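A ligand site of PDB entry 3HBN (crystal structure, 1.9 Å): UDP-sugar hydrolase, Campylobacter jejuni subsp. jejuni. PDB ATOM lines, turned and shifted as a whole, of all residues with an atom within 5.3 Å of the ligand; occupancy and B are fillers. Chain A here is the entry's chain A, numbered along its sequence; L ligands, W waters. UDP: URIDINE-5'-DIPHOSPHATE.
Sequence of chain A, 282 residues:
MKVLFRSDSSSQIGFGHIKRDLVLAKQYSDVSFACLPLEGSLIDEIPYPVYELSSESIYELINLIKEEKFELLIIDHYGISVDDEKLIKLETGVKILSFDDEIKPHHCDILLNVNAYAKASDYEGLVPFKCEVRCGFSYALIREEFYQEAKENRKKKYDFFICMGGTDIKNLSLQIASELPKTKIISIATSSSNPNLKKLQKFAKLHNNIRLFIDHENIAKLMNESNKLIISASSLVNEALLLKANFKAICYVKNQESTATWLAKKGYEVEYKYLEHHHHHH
The side-chain carboxylate (OE2) of Glu 239 is in salt-bridge range of the guanidinium group (NH1) of Arg 143 (3.8 Å).
The side-chain hydroxyl (OG) of Ser 234 sits at hydrogen-bond distance from the side-chain hydroxyl (OG) of Ser 232 (2.8 Å).
O of Gly 166 lies within hydrogen-bond range of OG of Ser 191 (2.6 Å).
The backbone NH (N) of Asp 215 lies within hydrogen-bond range of the backbone carbonyl oxygen (O) of Thr 190 (2.9 Å).
The backbone NH of Thr 190 lies within hydrogen-bond range of the backbone carbonyl oxygen of Phe 213 (3.1 Å).
The side-chain sulfur of Cys 163 sits at hydrogen-bond distance from the backbone carbonyl oxygen of Gly 165, 3.6 Å away.
The side-chain sulfur of Cys 163 lies within hydrogen-bond range of the backbone carbonyl oxygen of Ala 189.
O of Cys 163 is in hydrogen-bond range of N of Ser 232.
Merely in contact with the ligand: Gly 165, Gly 14, Ser 191, Cys 163, Ile 219, Ala 189 and Lys 19.
Hydrophobic or aromatic side chains that line the ligand: Phe 15, Ile 219 and Leu 236.
16 residues have an atom within 4 Å of the ligand: Gly 14, Phe 15, Gly 16, Lys 19, Arg 143, Cys 163, Gly 165, Gly 166, Ala 189, Thr 190, Ser 191, Ile 219, Ser 234, Ser 235, Leu 236 and Glu 239.
The nearest printed residue that does not touch the ligand is Phe 146 (4.1 Å).
Water W6 lies within hydrogen-bond range of O3B of the ligand (2.5 Å) and O of Ile 13 (3.1 Å).
Water W5 lies within hydrogen-bond range of O1B of the ligand (2.6 Å) and O of Ile 13 (3.0 Å).
Water W3 bridges O of His 216 (2.7 Å) and N3 of the ligand (2.7 Å).
Water W4 lies within hydrogen-bond range of O1B of the ligand, OG of Ser 232 and O of Met 164.
Water W8 lies within hydrogen-bond range of O1B of the ligand (2.9 Å), O of Met 164 (3.0 Å), N of Thr 167 (3.0 Å) and N of Gly 166 (3.2 Å).
Water W7 bridges an oxygen (O3') of the ligand (3.0 Å) and the side-chain hydroxyl (OG) of Ser 235 (3.2 Å).
An oxygen (O3') of the ligand is in hydrogen-bond range of the side-chain carboxylate (OE2) of Glu 239, 2.5 Å away.
O2A of the ligand sits at hydrogen-bond distance from OG of Ser 234 (2.6 Å).
An oxygen (O2B) of the ligand sits at hydrogen-bond distance from the backbone NH (N) of Phe 15.
An oxygen (O1A) of the ligand is in hydrogen-bond range of the backbone NH of Ser 235, 2.9 Å away.
The side-chain hydroxyl (OG) of Ser 235 sits at hydrogen-bond distance from an oxygen (O1A) of the ligand.
An oxygen (O2B) of the ligand is in hydrogen-bond range of the backbone NH (N) of Gly 166, at 2.8 Å.
N of Gly 16 is in hydrogen-bond range of O3B of the ligand (2.8 Å).
The guanidinium group (NH2) of Arg 143 lies within hydrogen-bond range of an oxygen (O2') of the ligand, at 2.8 Å.
An oxygen (O4) of the ligand lies close to the backbone NH (N) of Thr 190, 3.4 Å away.
The backbone NH of Leu 236 sits at hydrogen-bond distance from an oxygen (O2A) of the ligand (3.4 Å).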
ATOM      1  N   ILE A  13       6.403  19.151  -2.226  1.00  0.00           N
ATOM      2  CA  ILE A  13       6.667  20.154  -1.178  1.00  0.00           C
ATOM      3  C   ILE A  13       7.464  21.349  -1.695  1.00  0.00           C
ATOM      4  O   ILE A  13       7.281  22.480  -1.223  1.00  0.00           O
ATOM      5  CB  ILE A  13       7.397  19.492   0.027  1.00  0.00           C
ATOM      6  CG1 ILE A  13       6.395  18.614   0.793  1.00  0.00           C
ATOM      7  CG2 ILE A  13       8.049  20.550   0.954  1.00  0.00           C
ATOM      8  CD1 ILE A  13       7.043  17.674   1.819  1.00  0.00           C
ATOM      9  N   GLY A  14       8.336  21.099  -2.662  1.00  0.00           N
ATOM     10  CA  GLY A  14       9.270  22.106  -3.149  1.00  0.00           C
ATOM     11  C   GLY A  14      10.591  22.001  -2.433  1.00  0.00           C
ATOM     12  O   GLY A  14      10.804  21.090  -1.611  1.00  0.00           O
ATOM     13  N   PHE A  15      11.491  22.928  -2.743  1.00  0.00           N
ATOM     14  CA  PHE A  15      12.864  22.885  -2.261  1.00  0.00           C
ATOM     15  C   PHE A  15      13.159  23.959  -1.234  1.00  0.00           C
ATOM     16  O   PHE A  15      14.222  23.928  -0.607  1.00  0.00           O
ATOM     17  CB  PHE A  15      13.854  23.110  -3.412  1.00  0.00           C
ATOM     18  CG  PHE A  15      14.070  21.900  -4.304  1.00  0.00           C
ATOM     19  CD1 PHE A  15      13.451  20.680  -4.054  1.00  0.00           C
ATOM     20  CD2 PHE A  15      14.945  22.006  -5.390  1.00  0.00           C
ATOM     21  CE1 PHE A  15      13.689  19.569  -4.877  1.00  0.00           C
ATOM     22  CE2 PHE A  15      15.189  20.904  -6.224  1.00  0.00           C
ATOM     23  CZ  PHE A  15      14.552  19.687  -5.961  1.00  0.00           C
ATOM     24  N   GLY A  16      12.242  24.896  -1.081  1.00  0.00           N
ATOM     25  CA  GLY A  16      12.504  26.087  -0.281  1.00  0.00           C
ATOM     26  C   GLY A  16      12.912  25.810   1.152  1.00  0.00           C
ATOM     27  O   GLY A  16      13.834  26.471   1.675  1.00  0.00           O
ATOM     28  N   HIS A  17      12.245  24.860   1.807  1.00  0.00           N
ATOM     29  CA  HIS A  17      12.550  24.582   3.220  1.00  0.00           C
ATOM     30  C   HIS A  17      13.970  24.065   3.355  1.00  0.00           C
ATOM     31  O   HIS A  17      14.759  24.626   4.102  1.00  0.00           O
ATOM     32  CB  HIS A  17      11.583  23.567   3.866  1.00  0.00           C
ATOM     33  CG  HIS A  17      10.136  23.897   3.685  1.00  0.00           C
ATOM     34  ND1 HIS A  17       9.450  24.716   4.552  1.00  0.00           N
ATOM     35  CD2 HIS A  17       9.246  23.511   2.743  1.00  0.00           C
ATOM     36  CE1 HIS A  17       8.194  24.828   4.148  1.00  0.00           C
ATOM     37  NE2 HIS A  17       8.048  24.104   3.054  1.00  0.00           N
ATOM     38  N   LYS A  19      16.499  24.150   1.184  1.00  0.00           N
ATOM     39  CA  LYS A  19      17.530  25.077   0.716  1.00  0.00           C
ATOM     40  C   LYS A  19      17.845  26.163   1.744  1.00  0.00           C
ATOM     41  O   LYS A  19      19.033  26.456   2.009  1.00  0.00           O
ATOM     42  CB  LYS A  19      17.142  25.691  -0.627  1.00  0.00           C
ATOM     43  CG  LYS A  19      17.045  24.667  -1.739  1.00  0.00           C
ATOM     44  CD  LYS A  19      18.388  24.425  -2.368  1.00  0.00           C
ATOM     45  CE  LYS A  19      18.243  23.891  -3.800  1.00  0.00           C
ATOM     46  NZ  LYS A  19      19.603  23.485  -4.284  1.00  0.00           N
ATOM     47  N   ARG A 143      21.713  32.218  -0.242  1.00  0.00           N
ATOM     48  CA  ARG A 143      22.985  31.584  -0.588  1.00  0.00           C
ATOM     49  C   ARG A 143      24.075  32.588  -0.953  1.00  0.00           C
ATOM     50  O   ARG A 143      23.803  33.688  -1.458  1.00  0.00           O
ATOM     51  CB  ARG A 143      22.781  30.565  -1.728  1.00  0.00           C
ATOM     52  CG  ARG A 143      21.990  29.351  -1.307  1.00  0.00           C
ATOM     53  CD  ARG A 143      21.909  28.279  -2.399  1.00  0.00           C
ATOM     54  NE  ARG A 143      21.322  28.756  -3.651  1.00  0.00           N
ATOM     55  CZ  ARG A 143      20.018  28.842  -3.919  1.00  0.00           C
ATOM     56  NH1 ARG A 143      19.103  28.518  -3.007  1.00  0.00           N
ATOM     57  NH2 ARG A 143      19.628  29.274  -5.124  1.00  0.00           N
ATOM     58  N   PHE A 146      24.399  34.831  -4.235  1.00  0.00           N
ATOM     59  CA  PHE A 146      23.614  36.043  -4.422  1.00  0.00           C
ATOM     60  C   PHE A 146      24.353  37.266  -3.887  1.00  0.00           C
ATOM     61  O   PHE A 146      24.259  38.361  -4.446  1.00  0.00           O
ATOM     62  CB  PHE A 146      22.217  35.912  -3.782  1.00  0.00           C
ATOM     63  CG  PHE A 146      21.362  34.859  -4.433  1.00  0.00           C
ATOM     64  CD1 PHE A 146      21.401  33.542  -3.999  1.00  0.00           C
ATOM     65  CD2 PHE A 146      20.523  35.186  -5.503  1.00  0.00           C
ATOM     66  CE1 PHE A 146      20.618  32.556  -4.610  1.00  0.00           C
ATOM     67  CE2 PHE A 146      19.746  34.209  -6.123  1.00  0.00           C
ATOM     68  CZ  PHE A 146      19.789  32.893  -5.675  1.00  0.00           C
ATOM     69  N   CYS A 163      11.264  31.357 -13.038  1.00  0.00           N
ATOM     70  CA  CYS A 163      11.559  30.297 -12.091  1.00  0.00           C
ATOM     71  C   CYS A 163      10.397  30.194 -11.132  1.00  0.00           C
ATOM     72  O   CYS A 163      10.071  31.156 -10.450  1.00  0.00           O
ATOM     73  CB  CYS A 163      12.849  30.583 -11.308  1.00  0.00           C
ATOM     74  SG  CYS A 163      13.322  29.185 -10.304  1.00  0.00           S
ATOM     75  N   MET A 164       9.769  29.023 -11.112  1.00  0.00           N
ATOM     76  CA  MET A 164       8.605  28.826 -10.287  1.00  0.00           C
ATOM     77  C   MET A 164       8.971  28.063  -9.017  1.00  0.00           C
ATOM     78  O   MET A 164       8.134  27.395  -8.432  1.00  0.00           O
ATOM     79  CB  MET A 164       7.519  28.093 -11.074  1.00  0.00           C
ATOM     80  CG  MET A 164       6.840  28.933 -12.164  1.00  0.00           C
ATOM     81  SD  MET A 164       5.865  30.455 -11.388  1.00  0.00           S
ATOM     82  CE  MET A 164       7.019  31.909 -12.022  1.00  0.00           C
ATOM     83  N   GLY A 165      10.207  28.193  -8.579  1.00  0.00           N
ATOM     84  CA  GLY A 165      10.697  27.413  -7.434  1.00  0.00           C
ATOM     85  C   GLY A 165      11.448  26.174  -7.910  1.00  0.00           C
ATOM     86  O   GLY A 165      11.868  26.080  -9.082  1.00  0.00           O
ATOM     87  N   GLY A 166      11.631  25.220  -7.009  1.00  0.00           N
ATOM     88  CA  GLY A 166      12.397  24.027  -7.373  1.00  0.00           C
ATOM     89  C   GLY A 166      11.695  23.045  -8.305  1.00  0.00           C
ATOM     90  O   GLY A 166      12.351  22.393  -9.114  1.00  0.00           O
ATOM     91  N   THR A 167      10.379  22.939  -8.202  1.00  0.00           N
ATOM     92  CA  THR A 167       9.681  21.791  -8.792  1.00  0.00           C
ATOM     93  C   THR A 167       8.466  22.123  -9.658  1.00  0.00           C
ATOM     94  O   THR A 167       8.067  21.307 -10.499  1.00  0.00           O
ATOM     95  CB  THR A 167       9.249  20.797  -7.695  1.00  0.00           C
ATOM     96  OG1 THR A 167       8.318  21.425  -6.822  1.00  0.00           O
ATOM     97  CG2 THR A 167      10.469  20.329  -6.873  1.00  0.00           C
ATOM     98  N   ALA A 189      14.609  28.320 -15.289  1.00  0.00           N
ATOM     99  CA  ALA A 189      15.337  27.470 -14.353  1.00  0.00           C
ATOM    100  C   ALA A 189      14.382  26.544 -13.642  1.00  0.00           C
ATOM    101  O   ALA A 189      13.362  26.994 -13.102  1.00  0.00           O
ATOM    102  CB  ALA A 189      16.098  28.312 -13.334  1.00  0.00           C
ATOM    103  N   THR A 190      14.705  25.247 -13.651  1.00  0.00           N
ATOM    104  CA  THR A 190      13.972  24.282 -12.842  1.00  0.00           C
ATOM    105  C   THR A 190      14.885  23.133 -12.409  1.00  0.00           C
ATOM    106  O   THR A 190      16.039  23.038 -12.857  1.00  0.00           O
ATOM    107  CB  THR A 190      12.713  23.757 -13.559  1.00  0.00           C
ATOM    108  OG1 THR A 190      11.838  23.159 -12.605  1.00  0.00           O
ATOM    109  CG2 THR A 190      13.074  22.746 -14.634  1.00  0.00           C
ATOM    110  N   SER A 191      14.399  22.273 -11.526  1.00  0.00           N
ATOM    111  CA  SER A 191      15.194  21.127 -11.088  1.00  0.00           C
ATOM    112  C   SER A 191      14.753  19.825 -11.753  1.00  0.00           C
ATOM    113  O   SER A 191      13.668  19.750 -12.322  1.00  0.00           O
ATOM    114  CB  SER A 191      15.112  20.961  -9.572  1.00  0.00           C
ATOM    115  OG  SER A 191      13.909  20.337  -9.197  1.00  0.00           O
ATOM    116  N   PHE A 213      17.394  25.763 -18.163  1.00  0.00           N
ATOM    117  CA  PHE A 213      18.520  25.347 -17.331  1.00  0.00           C
ATOM    118  C   PHE A 213      18.042  24.422 -16.232  1.00  0.00           C
ATOM    119  O   PHE A 213      17.280  24.833 -15.346  1.00  0.00           O
ATOM    120  CB  PHE A 213      19.174  26.565 -16.696  1.00  0.00           C
ATOM    121  CG  PHE A 213      19.804  27.515 -17.673  1.00  0.00           C
ATOM    122  CD1 PHE A 213      19.119  28.662 -18.063  1.00  0.00           C
ATOM    123  CD2 PHE A 213      21.094  27.297 -18.146  1.00  0.00           C
ATOM    124  CE1 PHE A 213      19.691  29.570 -18.946  1.00  0.00           C
ATOM    125  CE2 PHE A 213      21.684  28.194 -19.048  1.00  0.00           C
ATOM    126  CZ  PHE A 213      20.989  29.340 -19.436  1.00  0.00           C
ATOM    127  N   ASP A 215      18.781  22.099 -12.963  1.00  0.00           N
ATOM    128  CA  ASP A 215      19.720  21.924 -11.845  1.00  0.00           C
ATOM    129  C   ASP A 215      20.929  22.860 -11.953  1.00  0.00           C
ATOM    130  O   ASP A 215      22.058  22.446 -11.684  1.00  0.00           O
ATOM    131  CB  ASP A 215      20.212  20.475 -11.762  1.00  0.00           C
ATOM    132  CG  ASP A 215      19.114  19.519 -11.391  1.00  0.00           C
ATOM    133  OD1 ASP A 215      18.140  19.943 -10.722  1.00  0.00           O
ATOM    134  OD2 ASP A 215      19.218  18.327 -11.747  1.00  0.00           O
ATOM    135  N   HIS A 216      20.687  24.104 -12.365  1.00  0.00           N
ATOM    136  CA  HIS A 216      21.749  25.095 -12.491  1.00  0.00           C
ATOM    137  C   HIS A 216      22.332  25.413 -11.111  1.00  0.00           C
ATOM    138  O   HIS A 216      21.601  25.483 -10.124  1.00  0.00           O
ATOM    139  CB  HIS A 216      21.218  26.370 -13.121  1.00  0.00           C
ATOM    140  CG  HIS A 216      22.283  27.312 -13.608  1.00  0.00           C
ATOM    141  ND1 HIS A 216      22.788  27.259 -14.890  1.00  0.00           N
ATOM    142  CD2 HIS A 216      22.908  28.336 -12.996  1.00  0.00           C
ATOM    143  CE1 HIS A 216      23.686  28.221 -15.046  1.00  0.00           C
ATOM    144  NE2 HIS A 216      23.785  28.891 -13.904  1.00  0.00           N
ATOM    145  N   ILE A 219      21.758  30.371  -9.615  1.00  0.00           N
ATOM    146  CA  ILE A 219      20.518  31.080  -9.927  1.00  0.00           C
ATOM    147  C   ILE A 219      20.744  32.590  -9.899  1.00  0.00           C
ATOM    148  O   ILE A 219      20.138  33.336 -10.658  1.00  0.00           O
ATOM    149  CB  ILE A 219      19.388  30.665  -8.944  1.00  0.00           C
ATOM    150  CG1 ILE A 219      19.040  29.172  -9.144  1.00  0.00           C
ATOM    151  CG2 ILE A 219      18.161  31.600  -9.030  1.00  0.00           C
ATOM    152  CD1 ILE A 219      18.491  28.825 -10.539  1.00  0.00           C
ATOM    153  N   SER A 232       7.913  32.767  -8.579  1.00  0.00           N
ATOM    154  CA  SER A 232       6.923  32.506  -7.522  1.00  0.00           C
ATOM    155  C   SER A 232       7.222  33.392  -6.307  1.00  0.00           C
ATOM    156  O   SER A 232       8.371  33.837  -6.128  1.00  0.00           O
ATOM    157  CB  SER A 232       6.865  31.023  -7.137  1.00  0.00           C
ATOM    158  OG  SER A 232       8.170  30.517  -6.916  1.00  0.00           O
ATOM    159  N   SER A 234       8.010  33.165  -3.304  1.00  0.00           N
ATOM    160  CA  SER A 234       8.609  32.178  -2.431  1.00  0.00           C
ATOM    161  C   SER A 234      10.006  32.669  -2.013  1.00  0.00           C
ATOM    162  O   SER A 234      10.257  33.888  -1.936  1.00  0.00           O
ATOM    163  CB  SER A 234       8.658  30.838  -3.198  1.00  0.00           C
ATOM    164  OG  SER A 234       9.368  30.988  -4.437  1.00  0.00           O
ATOM    165  N   SER A 235      10.937  31.749  -1.770  1.00  0.00           N
ATOM    166  CA  SER A 235      12.321  32.135  -1.430  1.00  0.00           C
ATOM    167  C   SER A 235      12.957  33.029  -2.494  1.00  0.00           C
ATOM    168  O   SER A 235      13.822  33.881  -2.188  1.00  0.00           O
ATOM    169  CB  SER A 235      13.221  30.898  -1.269  1.00  0.00           C
ATOM    170  OG  SER A 235      12.763  30.064  -0.212  1.00  0.00           O
ATOM    171  N   LEU A 236      12.522  32.829  -3.733  1.00  0.00           N
ATOM    172  CA  LEU A 236      13.037  33.573  -4.877  1.00  0.00           C
ATOM    173  C   LEU A 236      12.875  35.086  -4.716  1.00  0.00           C
ATOM    174  O   LEU A 236      13.676  35.848  -5.251  1.00  0.00           O
ATOM    175  CB  LEU A 236      12.327  33.118  -6.143  1.00  0.00           C
ATOM    176  CG  LEU A 236      12.683  31.714  -6.628  1.00  0.00           C
ATOM    177  CD1 LEU A 236      11.608  31.201  -7.565  1.00  0.00           C
ATOM    178  CD2 LEU A 236      14.066  31.697  -7.313  1.00  0.00           C
ATOM    179  N   GLU A 239      15.737  36.578  -2.710  1.00  0.00           N
ATOM    180  CA  GLU A 239      16.870  36.515  -3.605  1.00  0.00           C
ATOM    181  C   GLU A 239      16.834  37.668  -4.615  1.00  0.00           C
ATOM    182  O   GLU A 239      17.831  38.413  -4.779  1.00  0.00           O
ATOM    183  CB  GLU A 239      16.909  35.151  -4.286  1.00  0.00           C
ATOM    184  CG  GLU A 239      17.178  34.034  -3.260  1.00  0.00           C
ATOM    185  CD  GLU A 239      16.849  32.625  -3.745  1.00  0.00           C
ATOM    186  OE1 GLU A 239      16.443  32.432  -4.920  1.00  0.00           O
ATOM    187  OE2 GLU A 239      16.997  31.700  -2.932  1.00  0.00           O
HETATM  188  N1  UDP L   1      16.343  26.938  -7.052  1.00  0.00           N
HETATM  189  C2  UDP L   1      17.469  26.272  -7.543  1.00  0.00           C
HETATM  190  N3  UDP L   1      17.421  25.664  -8.786  1.00  0.00           N
HETATM  191  C4  UDP L   1      16.246  25.701  -9.527  1.00  0.00           C
HETATM  192  C5  UDP L   1      15.115  26.351  -9.033  1.00  0.00           C
HETATM  193  C6  UDP L   1      15.169  26.982  -7.786  1.00  0.00           C
HETATM  194  O2  UDP L   1      18.511  26.222  -6.894  1.00  0.00           O
HETATM  195  O4  UDP L   1      16.240  25.145 -10.638  1.00  0.00           O
HETATM  196  C1' UDP L   1      16.442  27.549  -5.714  1.00  0.00           C
HETATM  197  C2' UDP L   1      15.907  28.967  -5.582  1.00  0.00           C
HETATM  198  O2' UDP L   1      16.910  29.930  -5.673  1.00  0.00           O
HETATM  199  C3' UDP L   1      15.294  28.982  -4.190  1.00  0.00           C
HETATM  200  C4' UDP L   1      14.870  27.543  -3.985  1.00  0.00           C
HETATM  201  O4' UDP L   1      15.622  26.747  -4.896  1.00  0.00           O
HETATM  202  O3' UDP L   1      16.279  29.302  -3.199  1.00  0.00           O
HETATM  203  C5' UDP L   1      13.385  27.345  -4.241  1.00  0.00           C
HETATM  204  O5' UDP L   1      12.704  27.649  -3.039  1.00  0.00           O
HETATM  205  PA  UDP L   1      11.325  28.436  -3.129  1.00  0.00           P
HETATM  206  O1A UDP L   1      10.829  28.802  -1.773  1.00  0.00           O
HETATM  207  O2A UDP L   1      11.552  29.609  -4.005  1.00  0.00           O
HETATM  208  O3A UDP L   1      10.290  27.504  -3.926  1.00  0.00           O
HETATM  209  PB  UDP L   1       9.848  25.974  -3.666  1.00  0.00           P
HETATM  210  O1B UDP L   1       8.502  25.893  -4.252  1.00  0.00           O
HETATM  211  O2B UDP L   1      10.744  25.035  -4.359  1.00  0.00           O
HETATM  212  O3B UDP L   1       9.799  25.721  -2.206  1.00  0.00           O
HETATM  213  O   HOH W   1      21.327  26.567  -7.437  1.00  0.00           O
HETATM  214  O   HOH W   2      18.118  25.269 -12.740  1.00  0.00           O
HETATM  215  O   HOH W   3      19.557  24.031  -9.257  1.00  0.00           O
HETATM  216  O   HOH W   4       7.168  28.132  -5.329  1.00  0.00           O
HETATM  217  O   HOH W   5       6.514  24.706  -3.159  1.00  0.00           O
HETATM  218  O   HOH W   6       7.891  25.404  -0.601  1.00  0.00           O
HETATM  219  O   HOH W   7      15.692  28.870  -0.277  1.00  0.00           O
HETATM  220  O   HOH W   8       8.427  24.835  -6.938  1.00  0.00           O
